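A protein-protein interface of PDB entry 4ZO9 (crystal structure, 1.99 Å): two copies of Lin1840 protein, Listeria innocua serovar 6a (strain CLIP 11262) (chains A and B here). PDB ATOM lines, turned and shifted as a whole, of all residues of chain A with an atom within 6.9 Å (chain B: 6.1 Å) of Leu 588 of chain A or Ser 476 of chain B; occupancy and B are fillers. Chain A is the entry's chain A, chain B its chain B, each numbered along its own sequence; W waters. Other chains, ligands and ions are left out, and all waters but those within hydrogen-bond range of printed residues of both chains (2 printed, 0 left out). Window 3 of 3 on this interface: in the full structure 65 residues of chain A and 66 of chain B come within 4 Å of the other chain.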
ATOM      1  N   ARG A 582      11.504 -25.576  17.056  1.00  0.00           N
ATOM      2  CA  ARG A 582      12.727 -24.755  16.975  1.00  0.00           C
ATOM      3  C   ARG A 582      12.544 -23.354  17.614  1.00  0.00           C
ATOM      4  O   ARG A 582      13.316 -22.936  18.446  1.00  0.00           O
ATOM      5  CB  ARG A 582      13.145 -24.624  15.499  1.00  0.00           C
ATOM      6  CG  ARG A 582      14.269 -23.660  15.188  1.00  0.00           C
ATOM      7  CD  ARG A 582      15.648 -24.190  15.568  1.00  0.00           C
ATOM      8  NE  ARG A 582      16.699 -23.177  15.315  1.00  0.00           N
ATOM      9  CZ  ARG A 582      17.951 -23.443  14.939  1.00  0.00           C
ATOM     10  NH1 ARG A 582      18.823 -22.450  14.795  1.00  0.00           N
ATOM     11  NH2 ARG A 582      18.367 -24.682  14.721  1.00  0.00           N
ATOM     12  N   HIS A 586      15.190 -22.176  24.152  1.00  0.00           N
ATOM     13  CA  HIS A 586      15.885 -23.427  24.522  1.00  0.00           C
ATOM     14  C   HIS A 586      17.326 -23.387  24.047  1.00  0.00           C
ATOM     15  O   HIS A 586      17.735 -22.467  23.372  1.00  0.00           O
ATOM     16  CB  HIS A 586      15.179 -24.675  23.927  1.00  0.00           C
ATOM     17  CG  HIS A 586      15.401 -24.862  22.451  1.00  0.00           C
ATOM     18  ND1 HIS A 586      14.917 -23.991  21.504  1.00  0.00           N
ATOM     19  CD2 HIS A 586      16.061 -25.823  21.767  1.00  0.00           C
ATOM     20  CE1 HIS A 586      15.273 -24.408  20.298  1.00  0.00           C
ATOM     21  NE2 HIS A 586      15.964 -25.523  20.429  1.00  0.00           N
ATOM     22  N   TYR A 587      18.102 -24.359  24.513  1.00  0.00           N
ATOM     23  CA  TYR A 587      19.433 -24.615  24.038  1.00  0.00           C
ATOM     24  C   TYR A 587      19.399 -25.850  23.155  1.00  0.00           C
ATOM     25  O   TYR A 587      18.670 -26.805  23.425  1.00  0.00           O
ATOM     26  CB  TYR A 587      20.382 -24.916  25.189  1.00  0.00           C
ATOM     27  CG  TYR A 587      20.690 -23.793  26.123  1.00  0.00           C
ATOM     28  CD1 TYR A 587      21.603 -22.801  25.765  1.00  0.00           C
ATOM     29  CD2 TYR A 587      20.117 -23.742  27.408  1.00  0.00           C
ATOM     30  CE1 TYR A 587      21.910 -21.769  26.651  1.00  0.00           C
ATOM     31  CE2 TYR A 587      20.424 -22.726  28.294  1.00  0.00           C
ATOM     32  CZ  TYR A 587      21.339 -21.766  27.911  1.00  0.00           C
ATOM     33  OH  TYR A 587      21.609 -20.758  28.713  1.00  0.00           O
ATOM     34  N   LEU A 588      20.254 -25.860  22.152  1.00  0.00           N
ATOM     35  CA  LEU A 588      20.380 -27.013  21.275  1.00  0.00           C
ATOM     36  C   LEU A 588      21.029 -28.196  21.945  1.00  0.00           C
ATOM     37  O   LEU A 588      20.742 -29.321  21.545  1.00  0.00           O
ATOM     38  CB  LEU A 588      21.202 -26.674  20.042  1.00  0.00           C
ATOM     39  CG  LEU A 588      20.693 -25.569  19.174  1.00  0.00           C
ATOM     40  CD1 LEU A 588      21.743 -25.315  18.112  1.00  0.00           C
ATOM     41  CD2 LEU A 588      19.356 -25.946  18.563  1.00  0.00           C
ATOM     42  N   ASP A 589      21.883 -27.936  22.944  1.00  0.00           N
ATOM     43  CA  ASP A 589      22.732 -28.926  23.510  1.00  0.00           C
ATOM     44  C   ASP A 589      22.467 -29.314  24.977  1.00  0.00           C
ATOM     45  O   ASP A 589      22.993 -30.323  25.394  1.00  0.00           O
ATOM     46  CB  ASP A 589      24.245 -28.496  23.370  1.00  0.00           C
ATOM     47  CG  ASP A 589      24.587 -27.190  24.057  1.00  0.00           C
ATOM     48  OD1 ASP A 589      23.693 -26.338  24.213  1.00  0.00           O
ATOM     49  OD2 ASP A 589      25.773 -27.011  24.505  1.00  0.00           O
ATOM     50  N   ILE A 590      21.649 -28.566  25.730  1.00  0.00           N
ATOM     51  CA  ILE A 590      21.212 -28.972  27.098  1.00  0.00           C
ATOM     52  C   ILE A 590      19.748 -28.611  27.349  1.00  0.00           C
ATOM     53  O   ILE A 590      19.196 -27.833  26.597  1.00  0.00           O
ATOM     54  CB  ILE A 590      22.020 -28.272  28.197  1.00  0.00           C
ATOM     55  CG1 ILE A 590      21.860 -26.753  28.065  1.00  0.00           C
ATOM     56  CG2 ILE A 590      23.481 -28.683  28.078  1.00  0.00           C
ATOM     57  CD1 ILE A 590      22.356 -25.952  29.264  1.00  0.00           C
ATOM     58  N   PRO A 591      19.129 -29.193  28.371  1.00  0.00           N
ATOM     59  CA  PRO A 591      17.817 -28.764  28.871  1.00  0.00           C
ATOM     60  C   PRO A 591      17.810 -27.368  29.449  1.00  0.00           C
ATOM     61  O   PRO A 591      18.837 -26.913  29.972  1.00  0.00           O
ATOM     62  CB  PRO A 591      17.522 -29.776  30.001  1.00  0.00           C
ATOM     63  CG  PRO A 591      18.303 -30.984  29.639  1.00  0.00           C
ATOM     64  CD  PRO A 591      19.542 -30.476  28.960  1.00  0.00           C
ATOM     65  N   ARG B 146      27.410 -17.637  23.111  1.00  0.00           N
ATOM     66  CA  ARG B 146      26.423 -18.710  23.211  1.00  0.00           C
ATOM     67  C   ARG B 146      25.202 -18.441  22.350  1.00  0.00           C
ATOM     68  O   ARG B 146      24.584 -19.362  21.835  1.00  0.00           O
ATOM     69  CB  ARG B 146      25.981 -18.922  24.636  1.00  0.00           C
ATOM     70  CG  ARG B 146      27.065 -19.527  25.510  1.00  0.00           C
ATOM     71  CD  ARG B 146      26.609 -19.489  26.958  1.00  0.00           C
ATOM     72  NE  ARG B 146      26.638 -18.143  27.526  1.00  0.00           N
ATOM     73  CZ  ARG B 146      26.524 -17.839  28.816  1.00  0.00           C
ATOM     74  NH1 ARG B 146      26.327 -18.756  29.768  1.00  0.00           N
ATOM     75  NH2 ARG B 146      26.579 -16.579  29.164  1.00  0.00           N
ATOM     76  N   TRP B 147      24.843 -17.165  22.221  1.00  0.00           N
ATOM     77  CA  TRP B 147      23.655 -16.746  21.446  1.00  0.00           C
ATOM     78  C   TRP B 147      23.903 -16.980  19.973  1.00  0.00           C
ATOM     79  O   TRP B 147      24.913 -16.550  19.440  1.00  0.00           O
ATOM     80  CB  TRP B 147      23.449 -15.255  21.675  1.00  0.00           C
ATOM     81  CG  TRP B 147      22.112 -14.716  21.276  1.00  0.00           C
ATOM     82  CD1 TRP B 147      20.902 -15.210  21.621  1.00  0.00           C
ATOM     83  CD2 TRP B 147      21.874 -13.486  20.595  1.00  0.00           C
ATOM     84  NE1 TRP B 147      19.921 -14.393  21.154  1.00  0.00           N
ATOM     85  CE2 TRP B 147      20.485 -13.319  20.527  1.00  0.00           C
ATOM     86  CE3 TRP B 147      22.704 -12.521  20.026  1.00  0.00           C
ATOM     87  CZ2 TRP B 147      19.879 -12.220  19.882  1.00  0.00           C
ATOM     88  CZ3 TRP B 147      22.116 -11.412  19.382  1.00  0.00           C
ATOM     89  CH2 TRP B 147      20.718 -11.264  19.338  1.00  0.00           C
ATOM     90  N   GLY B 148      22.966 -17.651  19.292  1.00  0.00           N
ATOM     91  CA  GLY B 148      23.186 -18.063  17.914  1.00  0.00           C
ATOM     92  C   GLY B 148      23.152 -16.871  16.984  1.00  0.00           C
ATOM     93  O   GLY B 148      23.746 -16.898  15.908  1.00  0.00           O
ATOM     94  N   GLY B 202      22.893 -16.495  27.189  1.00  0.00           N
ATOM     95  CA  GLY B 202      22.867 -16.708  25.739  1.00  0.00           C
ATOM     96  C   GLY B 202      21.704 -17.482  25.206  1.00  0.00           C
ATOM     97  O   GLY B 202      21.739 -17.940  24.029  1.00  0.00           O
ATOM     98  N   LEU B 203      20.668 -17.617  26.046  1.00  0.00           N
ATOM     99  CA  LEU B 203      19.479 -18.381  25.714  1.00  0.00           C
ATOM    100  C   LEU B 203      18.525 -17.571  24.819  1.00  0.00           C
ATOM    101  O   LEU B 203      18.199 -16.446  25.090  1.00  0.00           O
ATOM    102  CB  LEU B 203      18.794 -18.823  27.025  1.00  0.00           C
ATOM    103  CG  LEU B 203      17.562 -19.672  26.995  1.00  0.00           C
ATOM    104  CD1 LEU B 203      17.891 -20.990  26.322  1.00  0.00           C
ATOM    105  CD2 LEU B 203      16.884 -19.924  28.373  1.00  0.00           C
ATOM    106  N   GLU B 204      18.080 -18.132  23.710  1.00  0.00           N
ATOM    107  CA  GLU B 204      17.218 -17.376  22.806  1.00  0.00           C
ATOM    108  C   GLU B 204      15.966 -16.833  23.488  1.00  0.00           C
ATOM    109  O   GLU B 204      15.270 -17.546  24.255  1.00  0.00           O
ATOM    110  CB  GLU B 204      16.844 -18.225  21.575  1.00  0.00           C
ATOM    111  CG  GLU B 204      16.264 -17.424  20.428  1.00  0.00           C
ATOM    112  CD  GLU B 204      17.235 -16.371  19.974  1.00  0.00           C
ATOM    113  OE1 GLU B 204      18.150 -16.746  19.187  1.00  0.00           O
ATOM    114  OE2 GLU B 204      17.110 -15.190  20.452  1.00  0.00           O
ATOM    115  N   TYR B 205      15.665 -15.572  23.160  1.00  0.00           N
ATOM    116  CA  TYR B 205      14.434 -14.842  23.621  1.00  0.00           C
ATOM    117  C   TYR B 205      14.483 -14.504  25.122  1.00  0.00           C
ATOM    118  O   TYR B 205      13.567 -13.909  25.649  1.00  0.00           O
ATOM    119  CB  TYR B 205      13.125 -15.560  23.289  1.00  0.00           C
ATOM    120  CG  TYR B 205      13.040 -16.123  21.847  1.00  0.00           C
ATOM    121  CD1 TYR B 205      13.163 -15.316  20.737  1.00  0.00           C
ATOM    122  CD2 TYR B 205      12.902 -17.507  21.621  1.00  0.00           C
ATOM    123  CE1 TYR B 205      13.064 -15.848  19.445  1.00  0.00           C
ATOM    124  CE2 TYR B 205      12.853 -18.044  20.323  1.00  0.00           C
ATOM    125  CZ  TYR B 205      12.968 -17.214  19.244  1.00  0.00           C
ATOM    126  OH  TYR B 205      12.900 -17.736  17.966  1.00  0.00           O
ATOM    127  N   GLU B 469      22.971 -24.474  11.112  1.00  0.00           N
ATOM    128  CA  GLU B 469      21.834 -24.699  11.982  1.00  0.00           C
ATOM    129  C   GLU B 469      22.187 -24.686  13.483  1.00  0.00           C
ATOM    130  O   GLU B 469      21.293 -24.596  14.299  1.00  0.00           O
ATOM    131  CB  GLU B 469      21.096 -25.992  11.614  1.00  0.00           C
ATOM    132  CG  GLU B 469      21.747 -27.279  12.085  1.00  0.00           C
ATOM    133  CD  GLU B 469      21.089 -28.520  11.549  1.00  0.00           C
ATOM    134  OE1 GLU B 469      20.955 -28.599  10.343  1.00  0.00           O
ATOM    135  OE2 GLU B 469      20.750 -29.435  12.321  1.00  0.00           O
ATOM    136  N   TRP B 470      23.467 -24.775  13.836  1.00  0.00           N
ATOM    137  CA  TRP B 470      23.862 -24.679  15.227  1.00  0.00           C
ATOM    138  C   TRP B 470      23.936 -23.224  15.765  1.00  0.00           C
ATOM    139  O   TRP B 470      24.373 -23.009  16.927  1.00  0.00           O
ATOM    140  CB  TRP B 470      25.187 -25.411  15.453  1.00  0.00           C
ATOM    141  CG  TRP B 470      25.138 -26.861  15.098  1.00  0.00           C
ATOM    142  CD1 TRP B 470      24.016 -27.665  15.037  1.00  0.00           C
ATOM    143  CD2 TRP B 470      26.253 -27.720  14.792  1.00  0.00           C
ATOM    144  NE1 TRP B 470      24.368 -28.944  14.688  1.00  0.00           N
ATOM    145  CE2 TRP B 470      25.731 -29.006  14.541  1.00  0.00           C
ATOM    146  CE3 TRP B 470      27.644 -27.540  14.771  1.00  0.00           C
ATOM    147  CZ2 TRP B 470      26.555 -30.104  14.190  1.00  0.00           C
ATOM    148  CZ3 TRP B 470      28.456 -28.634  14.456  1.00  0.00           C
ATOM    149  CH2 TRP B 470      27.898 -29.886  14.155  1.00  0.00           C
ATOM    150  N   GLY B 471      23.571 -22.263  14.898  1.00  0.00           N
ATOM    151  CA  GLY B 471      23.420 -20.880  15.203  1.00  0.00           C
ATOM    152  C   GLY B 471      22.307 -20.219  14.385  1.00  0.00           C
ATOM    153  O   GLY B 471      21.447 -20.900  13.858  1.00  0.00           O
ATOM    154  N   GLY B 472      22.343 -18.883  14.284  1.00  0.00           N
ATOM    155  CA  GLY B 472      21.193 -18.148  13.798  1.00  0.00           C
ATOM    156  C   GLY B 472      20.124 -18.099  14.883  1.00  0.00           C
ATOM    157  O   GLY B 472      20.434 -18.278  16.086  1.00  0.00           O
ATOM    158  N   GLU B 473      18.875 -17.824  14.496  1.00  0.00           N
ATOM    159  CA  GLU B 473      17.813 -17.716  15.486  1.00  0.00           C
ATOM    160  C   GLU B 473      17.531 -19.057  16.155  1.00  0.00           C
ATOM    161  O   GLU B 473      17.358 -20.097  15.474  1.00  0.00           O
ATOM    162  CB  GLU B 473      16.520 -17.142  14.898  1.00  0.00           C
ATOM    163  CG  GLU B 473      15.426 -16.905  15.957  1.00  0.00           C
ATOM    164  CD  GLU B 473      14.125 -16.299  15.387  1.00  0.00           C
ATOM    165  OE1 GLU B 473      14.171 -15.881  14.234  1.00  0.00           O
ATOM    166  OE2 GLU B 473      13.060 -16.248  16.075  1.00  0.00           O
ATOM    167  N   ALA B 474      17.538 -19.024  17.500  1.00  0.00           N
ATOM    168  CA  ALA B 474      17.108 -20.109  18.328  1.00  0.00           C
ATOM    169  C   ALA B 474      18.093 -21.261  18.132  1.00  0.00           C
ATOM    170  O   ALA B 474      17.745 -22.423  18.239  1.00  0.00           O
ATOM    171  CB  ALA B 474      15.627 -20.493  18.040  1.00  0.00           C
ATOM    172  N   GLY B 475      19.316 -20.874  17.805  1.00  0.00           N
ATOM    173  CA  GLY B 475      20.494 -21.732  17.768  1.00  0.00           C
ATOM    174  C   GLY B 475      21.467 -21.378  18.935  1.00  0.00           C
ATOM    175  O   GLY B 475      22.581 -21.002  18.714  1.00  0.00           O
ATOM    176  N   SER B 476      21.006 -21.584  20.154  1.00  0.00           N
ATOM    177  CA  SER B 476      21.705 -21.225  21.369  1.00  0.00           C
ATOM    178  C   SER B 476      22.501 -22.440  21.842  1.00  0.00           C
ATOM    179  O   SER B 476      21.962 -23.523  21.933  1.00  0.00           O
ATOM    180  CB  SER B 476      20.749 -20.745  22.466  1.00  0.00           C
ATOM    181  OG  SER B 476      20.232 -19.429  22.302  1.00  0.00           O
ATOM    182  N   LEU B 477      23.803 -22.264  22.106  1.00  0.00           N
ATOM    183  CA  LEU B 477      24.657 -23.356  22.587  1.00  0.00           C
ATOM    184  C   LEU B 477      25.156 -22.986  23.950  1.00  0.00           C
ATOM    185  O   LEU B 477      25.834 -21.957  24.101  1.00  0.00           O
ATOM    186  CB  LEU B 477      25.864 -23.556  21.716  1.00  0.00           C
ATOM    187  CG  LEU B 477      25.742 -24.263  20.389  1.00  0.00           C
ATOM    188  CD1 LEU B 477      27.144 -24.394  19.766  1.00  0.00           C
ATOM    189  CD2 LEU B 477      25.120 -25.640  20.588  1.00  0.00           C
ATOM    190  N   ALA B 478      24.867 -23.821  24.936  1.00  0.00           N
ATOM    191  CA  ALA B 478      25.464 -23.614  26.240  1.00  0.00           C
ATOM    192  C   ALA B 478      27.014 -23.698  26.282  1.00  0.00           C
ATOM    193  O   ALA B 478      27.660 -22.990  27.034  1.00  0.00           O
ATOM    194  CB  ALA B 478      24.843 -24.563  27.223  1.00  0.00           C
ATOM    195  N   ARG B 508      30.004 -18.175  15.153  1.00  0.00           N
ATOM    196  CA  ARG B 508      30.242 -17.651  16.501  1.00  0.00           C
ATOM    197  C   ARG B 508      31.673 -17.876  16.922  1.00  0.00           C
ATOM    198  O   ARG B 508      32.307 -18.848  16.500  1.00  0.00           O
ATOM    199  CB  ARG B 508      29.361 -18.351  17.524  1.00  0.00           C
ATOM    200  CG  ARG B 508      29.458 -19.881  17.480  1.00  0.00           C
ATOM    201  CD  ARG B 508      29.024 -20.621  18.736  1.00  0.00           C
ATOM    202  NE  ARG B 508      27.649 -20.347  19.120  1.00  0.00           N
ATOM    203  CZ  ARG B 508      26.566 -20.891  18.588  1.00  0.00           C
ATOM    204  NH1 ARG B 508      26.666 -21.759  17.589  1.00  0.00           N
ATOM    205  NH2 ARG B 508      25.352 -20.522  19.031  1.00  0.00           N
HETATM  206  O   HOH W   1      17.055 -20.914  12.953  1.00  0.00           O
HETATM  207  O   HOH W   2      18.629 -23.069  20.571  1.00  0.00           O
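Leu 588 of chain A touches just these residues of chain B: Glu 469, Trp 470, Ala 474, Gly 475 and Ser 476. Of the printed residues of chain A, Ser 476 of chain B touches His 586, Tyr 587 and Leu 588. Printed residues of chain B within 4 Å of Tyr 587 of chain A: Leu 203 (3.6 Å), Ser 476 (3.5 Å), Leu 477 (3.99 Å) and Ala 478 (3.5 Å). Printed residues of chain B within 4 Å of His 586 of chain A: Leu 203 (3.3 Å), Ala 474 (3.8 Å) and Ser 476 (3.6 Å). Printed residues of chain A within 4 Å of Ala 478 of chain B: Tyr 587, Asp 589 and Ile 590. Of the printed residues of chain B, Asp 589 of chain A touches Leu 477 and Ala 478. The nearest residue of chain B that does not touch Leu 588 of chain A is Leu 477 of chain B (4.1 Å). The nearest printed residue of chain A that does not touch Ser 476 of chain B is Asp 589 of chain A (4.01 Å). The nearest printed residue of chain B that does not touch Asp 589 of chain A is Ser 476 of chain B (4.01 Å).
Leu 203 of chain B touches His 586 of chain A. O of Ala 474 of chain B touches CE1 of His 586 of chain A, 3.8 Å away. Ser 476 of chain B touches His 586 of chain A (CB to O, 3.6 Å). Tyr 587 of chain A touches Ser 476 of chain B (CA to O, 3.5 Å). CD1 of Tyr 587 of chain A touches C of Leu 477 of chain B (3.99 Å). CD1 of Tyr 587 of chain A touches N of Ala 478 of chain B (3.5 Å). CD1 of Leu 588 of chain A touches CA of Trp 470 of chain B, at 3.6 Å. CD2 of Leu 588 of chain A touches O of Ala 474 of chain B (3.9 Å). CA of Gly 475 of chain B touches CD1 of Leu 588 of chain A, at 3.8 Å. Ile 590 of chain A touches Ala 478 of chain B.
The backbone NH of Gly 148 of chain B sits close to the backbone carbonyl oxygen of Gly 475 of chain B (3.4 Å). O of Gly 202 of chain B sits at hydrogen-bond distance from OG of Ser 476 of chain B (2.7 Å). The backbone NH of Ala 474 of chain B lies within hydrogen-bond range of the side-chain carboxylate of Glu 204 of chain B. The side-chain hydroxyl (OH) of Tyr 205 of chain B lies within hydrogen-bond range of the side-chain carboxylate (OE2) of Glu 473 of chain B (2.4 Å). O of Trp 470 of chain B is in hydrogen-bond range of NH1 of Arg 508 of chain B. O of Gly 475 of chain B is in hydrogen-bond range of NH2 of Arg 508 of chain B, 2.8 Å away.
Water W2 lies within hydrogen-bond range of the backbone carbonyl oxygen of Ala 474 of chain B, the backbone NH of Ser 476 of chain B and the backbone carbonyl oxygen of His 586 of chain A. Water W1 bridges O of Glu 473 of chain B (2.7 Å) and NH1 of Arg 582 of chain A (3.0 Å).
Hydrophobic or aromatic side chains of chain B within 4 Å of the printed part of chain A: Leu 203, Ala 474, Leu 477 and Ala 478. Of the 7 printed residues of chain A, 6 touch a printed residue of chain B. Among the printed residues, 20 pairs touch across the chains. Among the printed residues, no Asp or Glu carboxylate lies within 4 Å of a Lys or Arg side-chain nitrogen of the other chain.
No position is printed for both chains.
O of Glu 469 of chain B lies within hydrogen-bond range of NH2 of Arg 582 of chain A (3.0 Å). The guanidinium group of Arg 582 of chain A is in hydrogen-bond range of the backbone carbonyl oxygen of Gly 471 of chain B. The backbone carbonyl oxygen of Glu 473 of chain B is in hydrogen-bond range of the guanidinium group of Arg 582 of chain A. The guanidinium group (NE) of Arg 582 of chain A sits at hydrogen-bond distance from the backbone carbonyl oxygen (O) of Ala 474 of chain B (3.2 Å). The backbone carbonyl oxygen (O) of Ser 476 of chain B lies within hydrogen-bond range of the backbone NH (N) of Leu 588 of chain A, 2.9 Å away. The backbone NH (N) of Ala 478 of chain B sits at hydrogen-bond distance from the side-chain carboxylate (OD1) of Asp 589 of chain A (2.9 Å). NH1 of Arg 582 of chain A lies close to N of Gly 475 of chain B.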
